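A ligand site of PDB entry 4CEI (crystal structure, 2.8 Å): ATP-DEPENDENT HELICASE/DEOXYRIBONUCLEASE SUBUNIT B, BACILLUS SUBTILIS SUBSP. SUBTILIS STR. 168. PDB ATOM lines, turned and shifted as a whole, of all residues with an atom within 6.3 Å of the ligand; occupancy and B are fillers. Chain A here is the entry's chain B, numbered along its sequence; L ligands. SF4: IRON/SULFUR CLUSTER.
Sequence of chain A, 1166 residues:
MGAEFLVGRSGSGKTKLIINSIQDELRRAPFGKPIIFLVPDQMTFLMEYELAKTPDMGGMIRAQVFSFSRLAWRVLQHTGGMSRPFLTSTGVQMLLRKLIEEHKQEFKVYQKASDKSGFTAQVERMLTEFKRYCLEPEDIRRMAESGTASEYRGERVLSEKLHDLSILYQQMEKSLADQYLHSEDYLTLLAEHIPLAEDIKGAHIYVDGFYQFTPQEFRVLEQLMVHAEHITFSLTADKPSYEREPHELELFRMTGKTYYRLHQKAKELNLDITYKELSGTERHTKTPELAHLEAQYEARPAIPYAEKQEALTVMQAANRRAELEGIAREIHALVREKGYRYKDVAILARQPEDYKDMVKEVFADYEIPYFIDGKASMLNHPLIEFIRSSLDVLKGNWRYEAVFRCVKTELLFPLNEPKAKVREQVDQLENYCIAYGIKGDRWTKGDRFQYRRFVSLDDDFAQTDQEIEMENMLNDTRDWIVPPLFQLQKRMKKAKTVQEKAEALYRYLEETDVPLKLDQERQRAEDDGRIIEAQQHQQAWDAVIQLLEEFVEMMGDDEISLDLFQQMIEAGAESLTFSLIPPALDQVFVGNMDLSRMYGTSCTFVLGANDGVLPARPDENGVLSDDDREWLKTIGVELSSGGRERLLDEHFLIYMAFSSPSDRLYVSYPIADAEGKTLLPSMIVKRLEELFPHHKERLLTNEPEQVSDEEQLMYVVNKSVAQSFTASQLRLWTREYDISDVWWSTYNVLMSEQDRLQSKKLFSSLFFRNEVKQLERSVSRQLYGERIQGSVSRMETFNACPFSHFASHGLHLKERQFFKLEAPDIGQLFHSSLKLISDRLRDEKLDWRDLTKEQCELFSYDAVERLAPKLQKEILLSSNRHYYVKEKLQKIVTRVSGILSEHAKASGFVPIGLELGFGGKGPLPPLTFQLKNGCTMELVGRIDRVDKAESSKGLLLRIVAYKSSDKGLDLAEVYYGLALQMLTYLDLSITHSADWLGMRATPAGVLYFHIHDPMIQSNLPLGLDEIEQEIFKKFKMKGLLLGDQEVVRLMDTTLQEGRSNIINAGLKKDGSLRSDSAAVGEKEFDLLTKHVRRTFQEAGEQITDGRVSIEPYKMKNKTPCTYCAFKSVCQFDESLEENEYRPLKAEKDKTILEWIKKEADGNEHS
Residues that only touch the ligand: Pro 1112, Ile 1110, Lys 1127, Ser 804, Phe 1126 and Pro 1120.
Hydrophobic or aromatic side chains that line the ligand: Ile 1110, Pro 1112 and Pro 1120.
Ten residues have an atom within 4 Å of the ligand: Cys 801, Ser 804, Ile 1110, Pro 1112, Pro 1120, Cys 1121, Cys 1124, Phe 1126, Lys 1127 and Cys 1130.
An iron atom (FE3) of the ligand is bound by the side-chain sulfur (SG) of Cys 1130 (2.3 Å).
An iron atom (FE4) of the ligand is bound by the side-chain sulfur of Cys 1124 (2.3 Å).
The side-chain sulfur (SG) of Cys 801 binds an iron atom (FE1) of the ligand, at 2.3 Å.
The side-chain sulfur (SG) of Cys 1121 is bound to an iron atom (FE2) of the ligand, at 2.3 Å.
The side-chain sulfur of Cys 1130 lies close to the backbone carbonyl oxygen of Lys 1127.
The backbone carbonyl oxygen of Phe 1126 sits close to the side-chain sulfur of Cys 1130.
SG of Cys 1130 sits close to N of Phe 1132 (3.3 Å).
SG of Cys 1124 sits close to N of Phe 1126, 3.5 Å away.
The side-chain hydroxyl (OG) of Ser 804 is in hydrogen-bond range of the backbone carbonyl oxygen (O) of Cys 801, 2.5 Å away.
SG of Cys 801 lies close to N of Phe 803, 3.5 Å away.
The backbone NH of Glu 1111 sits close to the side-chain sulfur of Cys 801, at 3.7 Å.
O of Cys 1121 is in hydrogen-bond range of NZ of Lys 1127 (3.1 Å).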
ATOM      1  N   ALA A 800       7.002 -15.758  -4.588  1.00  0.00           N
ATOM      2  CA  ALA A 800       6.521 -14.410  -4.870  1.00  0.00           C
ATOM      3  C   ALA A 800       5.330 -14.490  -5.806  1.00  0.00           C
ATOM      4  O   ALA A 800       4.293 -13.863  -5.576  1.00  0.00           O
ATOM      5  CB  ALA A 800       7.627 -13.556  -5.460  1.00  0.00           C
ATOM      6  N   CYS A 801       5.498 -15.269  -6.863  1.00  0.00           N
ATOM      7  CA  CYS A 801       4.469 -15.463  -7.874  1.00  0.00           C
ATOM      8  C   CYS A 801       4.839 -16.634  -8.754  1.00  0.00           C
ATOM      9  O   CYS A 801       5.864 -16.587  -9.443  1.00  0.00           O
ATOM     10  CB  CYS A 801       4.290 -14.194  -8.711  1.00  0.00           C
ATOM     11  SG  CYS A 801       3.320 -14.415 -10.220  1.00  0.00           S
ATOM     12  N   PRO A 802       4.015 -17.698  -8.734  1.00  0.00           N
ATOM     13  CA  PRO A 802       4.298 -18.887  -9.542  1.00  0.00           C
ATOM     14  C   PRO A 802       4.514 -18.564 -11.022  1.00  0.00           C
ATOM     15  O   PRO A 802       5.418 -19.140 -11.625  1.00  0.00           O
ATOM     16  CB  PRO A 802       3.040 -19.753  -9.352  1.00  0.00           C
ATOM     17  CG  PRO A 802       2.498 -19.327  -8.042  1.00  0.00           C
ATOM     18  CD  PRO A 802       2.775 -17.854  -7.957  1.00  0.00           C
ATOM     19  N   PHE A 803       3.722 -17.652 -11.572  1.00  0.00           N
ATOM     20  CA  PHE A 803       3.872 -17.317 -12.979  1.00  0.00           C
ATOM     21  C   PHE A 803       5.243 -16.718 -13.280  1.00  0.00           C
ATOM     22  O   PHE A 803       5.884 -17.079 -14.272  1.00  0.00           O
ATOM     23  CB  PHE A 803       2.798 -16.340 -13.436  1.00  0.00           C
ATOM     24  CG  PHE A 803       2.723 -16.181 -14.928  1.00  0.00           C
ATOM     25  CD1 PHE A 803       3.508 -15.241 -15.575  1.00  0.00           C
ATOM     26  CD2 PHE A 803       1.895 -16.995 -15.683  1.00  0.00           C
ATOM     27  CE1 PHE A 803       3.449 -15.104 -16.942  1.00  0.00           C
ATOM     28  CE2 PHE A 803       1.835 -16.868 -17.053  1.00  0.00           C
ATOM     29  CZ  PHE A 803       2.613 -15.919 -17.693  1.00  0.00           C
ATOM     30  N   SER A 804       5.685 -15.789 -12.432  1.00  0.00           N
ATOM     31  CA  SER A 804       6.987 -15.161 -12.616  1.00  0.00           C
ATOM     32  C   SER A 804       8.073 -16.236 -12.625  1.00  0.00           C
ATOM     33  O   SER A 804       9.016 -16.160 -13.415  1.00  0.00           O
ATOM     34  CB  SER A 804       7.256 -14.131 -11.527  1.00  0.00           C
ATOM     35  OG  SER A 804       7.310 -14.734 -10.251  1.00  0.00           O
ATOM     36  N   SER A1109       0.421 -20.451 -11.708  1.00  0.00           N
ATOM     37  CA  SER A1109      -0.642 -19.462 -11.543  1.00  0.00           C
ATOM     38  C   SER A1109      -0.133 -18.052 -11.230  1.00  0.00           C
ATOM     39  O   SER A1109       0.869 -17.884 -10.544  1.00  0.00           O
ATOM     40  CB  SER A1109      -1.610 -19.906 -10.443  1.00  0.00           C
ATOM     41  OG  SER A1109      -0.899 -20.204  -9.247  1.00  0.00           O
ATOM     42  N   ILE A1110      -0.832 -17.048 -11.756  1.00  0.00           N
ATOM     43  CA  ILE A1110      -0.490 -15.652 -11.520  1.00  0.00           C
ATOM     44  C   ILE A1110      -1.022 -15.211 -10.163  1.00  0.00           C
ATOM     45  O   ILE A1110      -2.187 -14.836 -10.035  1.00  0.00           O
ATOM     46  CB  ILE A1110      -1.064 -14.749 -12.627  1.00  0.00           C
ATOM     47  CG1 ILE A1110      -0.603 -15.232 -14.001  1.00  0.00           C
ATOM     48  CG2 ILE A1110      -0.672 -13.282 -12.390  1.00  0.00           C
ATOM     49  CD1 ILE A1110      -1.191 -14.448 -15.158  1.00  0.00           C
ATOM     50  N   GLU A1111      -0.170 -15.260  -9.143  1.00  0.00           N
ATOM     51  CA  GLU A1111      -0.588 -14.909  -7.794  1.00  0.00           C
ATOM     52  C   GLU A1111       0.392 -13.982  -7.095  1.00  0.00           C
ATOM     53  O   GLU A1111       1.157 -14.415  -6.235  1.00  0.00           O
ATOM     54  CB  GLU A1111      -0.782 -16.183  -6.951  1.00  0.00           C
ATOM     55  CG  GLU A1111      -1.993 -17.005  -7.344  1.00  0.00           C
ATOM     56  CD  GLU A1111      -2.030 -18.355  -6.654  1.00  0.00           C
ATOM     57  OE1 GLU A1111      -0.993 -18.765  -6.085  1.00  0.00           O
ATOM     58  OE2 GLU A1111      -3.095 -18.996  -6.675  1.00  0.00           O
ATOM     59  N   PRO A1112       0.374 -12.694  -7.462  1.00  0.00           N
ATOM     60  CA  PRO A1112       1.228 -11.673  -6.855  1.00  0.00           C
ATOM     61  C   PRO A1112       0.829 -11.411  -5.406  1.00  0.00           C
ATOM     62  O   PRO A1112      -0.355 -11.334  -5.111  1.00  0.00           O
ATOM     63  CB  PRO A1112       0.993 -10.423  -7.718  1.00  0.00           C
ATOM     64  CG  PRO A1112       0.147 -10.876  -8.881  1.00  0.00           C
ATOM     65  CD  PRO A1112      -0.550 -12.121  -8.450  1.00  0.00           C
ATOM     66  N   THR A1119       4.835  -5.025  -3.640  1.00  0.00           N
ATOM     67  CA  THR A1119       4.485  -6.167  -4.471  1.00  0.00           C
ATOM     68  C   THR A1119       5.727  -6.669  -5.214  1.00  0.00           C
ATOM     69  O   THR A1119       6.705  -5.931  -5.338  1.00  0.00           O
ATOM     70  CB  THR A1119       3.392  -5.800  -5.500  1.00  0.00           C
ATOM     71  OG1 THR A1119       3.976  -5.064  -6.595  1.00  0.00           O
ATOM     72  CG2 THR A1119       2.288  -4.969  -4.856  1.00  0.00           C
ATOM     73  N   PRO A1120       5.707  -7.926  -5.686  1.00  0.00           N
ATOM     74  CA  PRO A1120       6.858  -8.394  -6.477  1.00  0.00           C
ATOM     75  C   PRO A1120       6.838  -7.819  -7.898  1.00  0.00           C
ATOM     76  O   PRO A1120       7.857  -7.855  -8.591  1.00  0.00           O
ATOM     77  CB  PRO A1120       6.658  -9.906  -6.497  1.00  0.00           C
ATOM     78  CG  PRO A1120       5.186 -10.085  -6.414  1.00  0.00           C
ATOM     79  CD  PRO A1120       4.711  -8.995  -5.489  1.00  0.00           C
ATOM     80  N   CYS A1121       5.693  -7.280  -8.296  1.00  0.00           N
ATOM     81  CA  CYS A1121       5.478  -6.795  -9.655  1.00  0.00           C
ATOM     82  C   CYS A1121       6.392  -5.627 -10.034  1.00  0.00           C
ATOM     83  O   CYS A1121       6.823  -5.518 -11.182  1.00  0.00           O
ATOM     84  CB  CYS A1121       4.018  -6.375  -9.847  1.00  0.00           C
ATOM     85  SG  CYS A1121       2.845  -7.619  -9.276  1.00  0.00           S
ATOM     86  N   THR A1122       6.662  -4.758  -9.065  1.00  0.00           N
ATOM     87  CA  THR A1122       7.492  -3.579  -9.268  1.00  0.00           C
ATOM     88  C   THR A1122       8.846  -3.910  -9.884  1.00  0.00           C
ATOM     89  O   THR A1122       9.337  -3.190 -10.751  1.00  0.00           O
ATOM     90  CB  THR A1122       7.715  -2.825  -7.944  1.00  0.00           C
ATOM     91  OG1 THR A1122       6.452  -2.478  -7.366  1.00  0.00           O
ATOM     92  CG2 THR A1122       8.542  -1.567  -8.163  1.00  0.00           C
ATOM     93  N   CYS A1124       9.532  -6.851 -11.454  1.00  0.00           N
ATOM     94  CA  CYS A1124       9.378  -8.009 -12.318  1.00  0.00           C
ATOM     95  C   CYS A1124       9.328  -7.646 -13.792  1.00  0.00           C
ATOM     96  O   CYS A1124       8.578  -6.770 -14.212  1.00  0.00           O
ATOM     97  CB  CYS A1124       8.139  -8.795 -11.930  1.00  0.00           C
ATOM     98  SG  CYS A1124       7.951 -10.330 -12.859  1.00  0.00           S
ATOM     99  N   ALA A1125      10.123  -8.362 -14.582  1.00  0.00           N
ATOM    100  CA  ALA A1125      10.245  -8.092 -16.012  1.00  0.00           C
ATOM    101  C   ALA A1125       9.036  -8.564 -16.816  1.00  0.00           C
ATOM    102  O   ALA A1125       8.858  -8.163 -17.965  1.00  0.00           O
ATOM    103  CB  ALA A1125      11.520  -8.741 -16.543  1.00  0.00           C
ATOM    104  N   PHE A1126       8.202  -9.392 -16.207  1.00  0.00           N
ATOM    105  CA  PHE A1126       7.191 -10.138 -16.964  1.00  0.00           C
ATOM    106  C   PHE A1126       5.771  -9.586 -16.833  1.00  0.00           C
ATOM    107  O   PHE A1126       4.796 -10.311 -17.035  1.00  0.00           O
ATOM    108  CB  PHE A1126       7.218 -11.596 -16.536  1.00  0.00           C
ATOM    109  CG  PHE A1126       8.587 -12.206 -16.546  1.00  0.00           C
ATOM    110  CD1 PHE A1126       9.261 -12.383 -17.745  1.00  0.00           C
ATOM    111  CD2 PHE A1126       9.211 -12.589 -15.362  1.00  0.00           C
ATOM    112  CE1 PHE A1126      10.532 -12.939 -17.769  1.00  0.00           C
ATOM    113  CE2 PHE A1126      10.482 -13.144 -15.386  1.00  0.00           C
ATOM    114  CZ  PHE A1126      11.133 -13.320 -16.585  1.00  0.00           C
ATOM    115  N   LYS A1127       5.660  -8.297 -16.519  1.00  0.00           N
ATOM    116  CA  LYS A1127       4.363  -7.670 -16.326  1.00  0.00           C
ATOM    117  C   LYS A1127       3.501  -7.696 -17.593  1.00  0.00           C
ATOM    118  O   LYS A1127       2.278  -7.780 -17.503  1.00  0.00           O
ATOM    119  CB  LYS A1127       4.533  -6.223 -15.856  1.00  0.00           C
ATOM    120  CG  LYS A1127       3.231  -5.532 -15.472  1.00  0.00           C
ATOM    121  CD  LYS A1127       3.241  -5.024 -14.029  1.00  0.00           C
ATOM    122  CE  LYS A1127       4.105  -3.780 -13.836  1.00  0.00           C
ATOM    123  NZ  LYS A1127       5.557  -4.082 -13.619  1.00  0.00           N
ATOM    124  N   SER A1128       4.139  -7.629 -18.754  1.00  0.00           N
ATOM    125  CA  SER A1128       3.383  -7.627 -20.003  1.00  0.00           C
ATOM    126  C   SER A1128       3.135  -9.036 -20.538  1.00  0.00           C
ATOM    127  O   SER A1128       2.408  -9.212 -21.515  1.00  0.00           O
ATOM    128  CB  SER A1128       4.116  -6.806 -21.069  1.00  0.00           C
ATOM    129  OG  SER A1128       5.244  -7.498 -21.567  1.00  0.00           O
ATOM    130  N   VAL A1129       3.727 -10.031 -19.885  1.00  0.00           N
ATOM    131  CA  VAL A1129       3.484 -11.427 -20.241  1.00  0.00           C
ATOM    132  C   VAL A1129       2.295 -11.954 -19.439  1.00  0.00           C
ATOM    133  O   VAL A1129       1.377 -12.542 -19.994  1.00  0.00           O
ATOM    134  CB  VAL A1129       4.706 -12.311 -19.998  1.00  0.00           C
ATOM    135  CG1 VAL A1129       4.435 -13.723 -20.488  1.00  0.00           C
ATOM    136  CG2 VAL A1129       5.934 -11.741 -20.685  1.00  0.00           C
ATOM    137  N   CYS A1130       2.333 -11.741 -18.131  1.00  0.00           N
ATOM    138  CA  CYS A1130       1.236 -12.122 -17.250  1.00  0.00           C
ATOM    139  C   CYS A1130      -0.031 -11.363 -17.611  1.00  0.00           C
ATOM    140  O   CYS A1130      -1.126 -11.941 -17.592  1.00  0.00           O
ATOM    141  CB  CYS A1130       1.600 -11.855 -15.800  1.00  0.00           C
ATOM    142  SG  CYS A1130       1.637 -10.100 -15.397  1.00  0.00           S
ATOM    143  N   GLN A1131       0.121 -10.082 -17.900  1.00  0.00           N
ATOM    144  CA  GLN A1131      -0.988  -9.200 -18.257  1.00  0.00           C
ATOM    145  C   GLN A1131      -1.989  -9.136 -17.116  1.00  0.00           C
ATOM    146  O   GLN A1131      -3.200  -9.035 -17.327  1.00  0.00           O
ATOM    147  CB  GLN A1131      -1.633  -9.664 -19.560  1.00  0.00           C
ATOM    148  CG  GLN A1131      -0.618  -9.828 -20.687  1.00  0.00           C
ATOM    149  CD  GLN A1131      -1.160 -10.568 -21.885  1.00  0.00           C
ATOM    150  OE1 GLN A1131      -2.367 -10.751 -22.040  1.00  0.00           O
ATOM    151  NE2 GLN A1131      -0.258 -11.011 -22.755  1.00  0.00           N
ATOM    152  N   PHE A1132      -1.461  -9.197 -15.894  1.00  0.00           N
ATOM    153  CA  PHE A1132      -2.225  -9.087 -14.663  1.00  0.00           C
ATOM    154  C   PHE A1132      -3.101  -7.840 -14.646  1.00  0.00           C
ATOM    155  O   PHE A1132      -2.599  -6.720 -14.757  1.00  0.00           O
ATOM    156  CB  PHE A1132      -1.262  -9.087 -13.468  1.00  0.00           C
ATOM    157  CG  PHE A1132      -1.922  -8.967 -12.133  1.00  0.00           C
ATOM    158  CD1 PHE A1132      -2.373 -10.099 -11.463  1.00  0.00           C
ATOM    159  CD2 PHE A1132      -2.066  -7.735 -11.518  1.00  0.00           C
ATOM    160  CE1 PHE A1132      -2.976  -9.995 -10.221  1.00  0.00           C
ATOM    161  CE2 PHE A1132      -2.655  -7.623 -10.268  1.00  0.00           C
ATOM    162  CZ  PHE A1132      -3.106  -8.758  -9.623  1.00  0.00           C
ATOM    163  N   TYR A1141      -4.327  -9.518  -5.952  1.00  0.00           N
ATOM    164  CA  TYR A1141      -3.124  -9.689  -5.151  1.00  0.00           C
ATOM    165  C   TYR A1141      -3.393 -10.589  -3.956  1.00  0.00           C
ATOM    166  O   TYR A1141      -4.528 -10.743  -3.523  1.00  0.00           O
ATOM    167  CB  TYR A1141      -2.602  -8.334  -4.678  1.00  0.00           C
ATOM    168  CG  TYR A1141      -2.139  -7.415  -5.786  1.00  0.00           C
ATOM    169  CD1 TYR A1141      -0.868  -7.541  -6.331  1.00  0.00           C
ATOM    170  CD2 TYR A1141      -2.970  -6.430  -6.289  1.00  0.00           C
ATOM    171  CE1 TYR A1141      -0.439  -6.707  -7.336  1.00  0.00           C
ATOM    172  CE2 TYR A1141      -2.554  -5.594  -7.299  1.00  0.00           C
ATOM    173  CZ  TYR A1141      -1.284  -5.727  -7.823  1.00  0.00           C
ATOM    174  OH  TYR A1141      -0.881  -4.888  -8.837  1.00  0.00           O
HETATM  175 FE1  SF4 L   1       3.502 -12.324 -11.162  1.00  0.00          FE
HETATM  176 FE2  SF4 L   1       3.391  -9.271 -10.811  1.00  0.00          FE
HETATM  177 FE3  SF4 L   1       2.983 -10.507 -13.614  1.00  0.00          FE
HETATM  178 FE4  SF4 L   1       5.756 -10.542 -12.290  1.00  0.00          FE
HETATM  179  S1  SF4 L   1       4.302  -8.977 -12.774  1.00  0.00           S
HETATM  180  S2  SF4 L   1       4.438 -12.064 -13.127  1.00  0.00           S
HETATM  181  S3  SF4 L   1       4.846 -10.818 -10.320  1.00  0.00           S
HETATM  182  S4  SF4 L   1       2.043 -10.765 -11.658  1.00  0.00           S
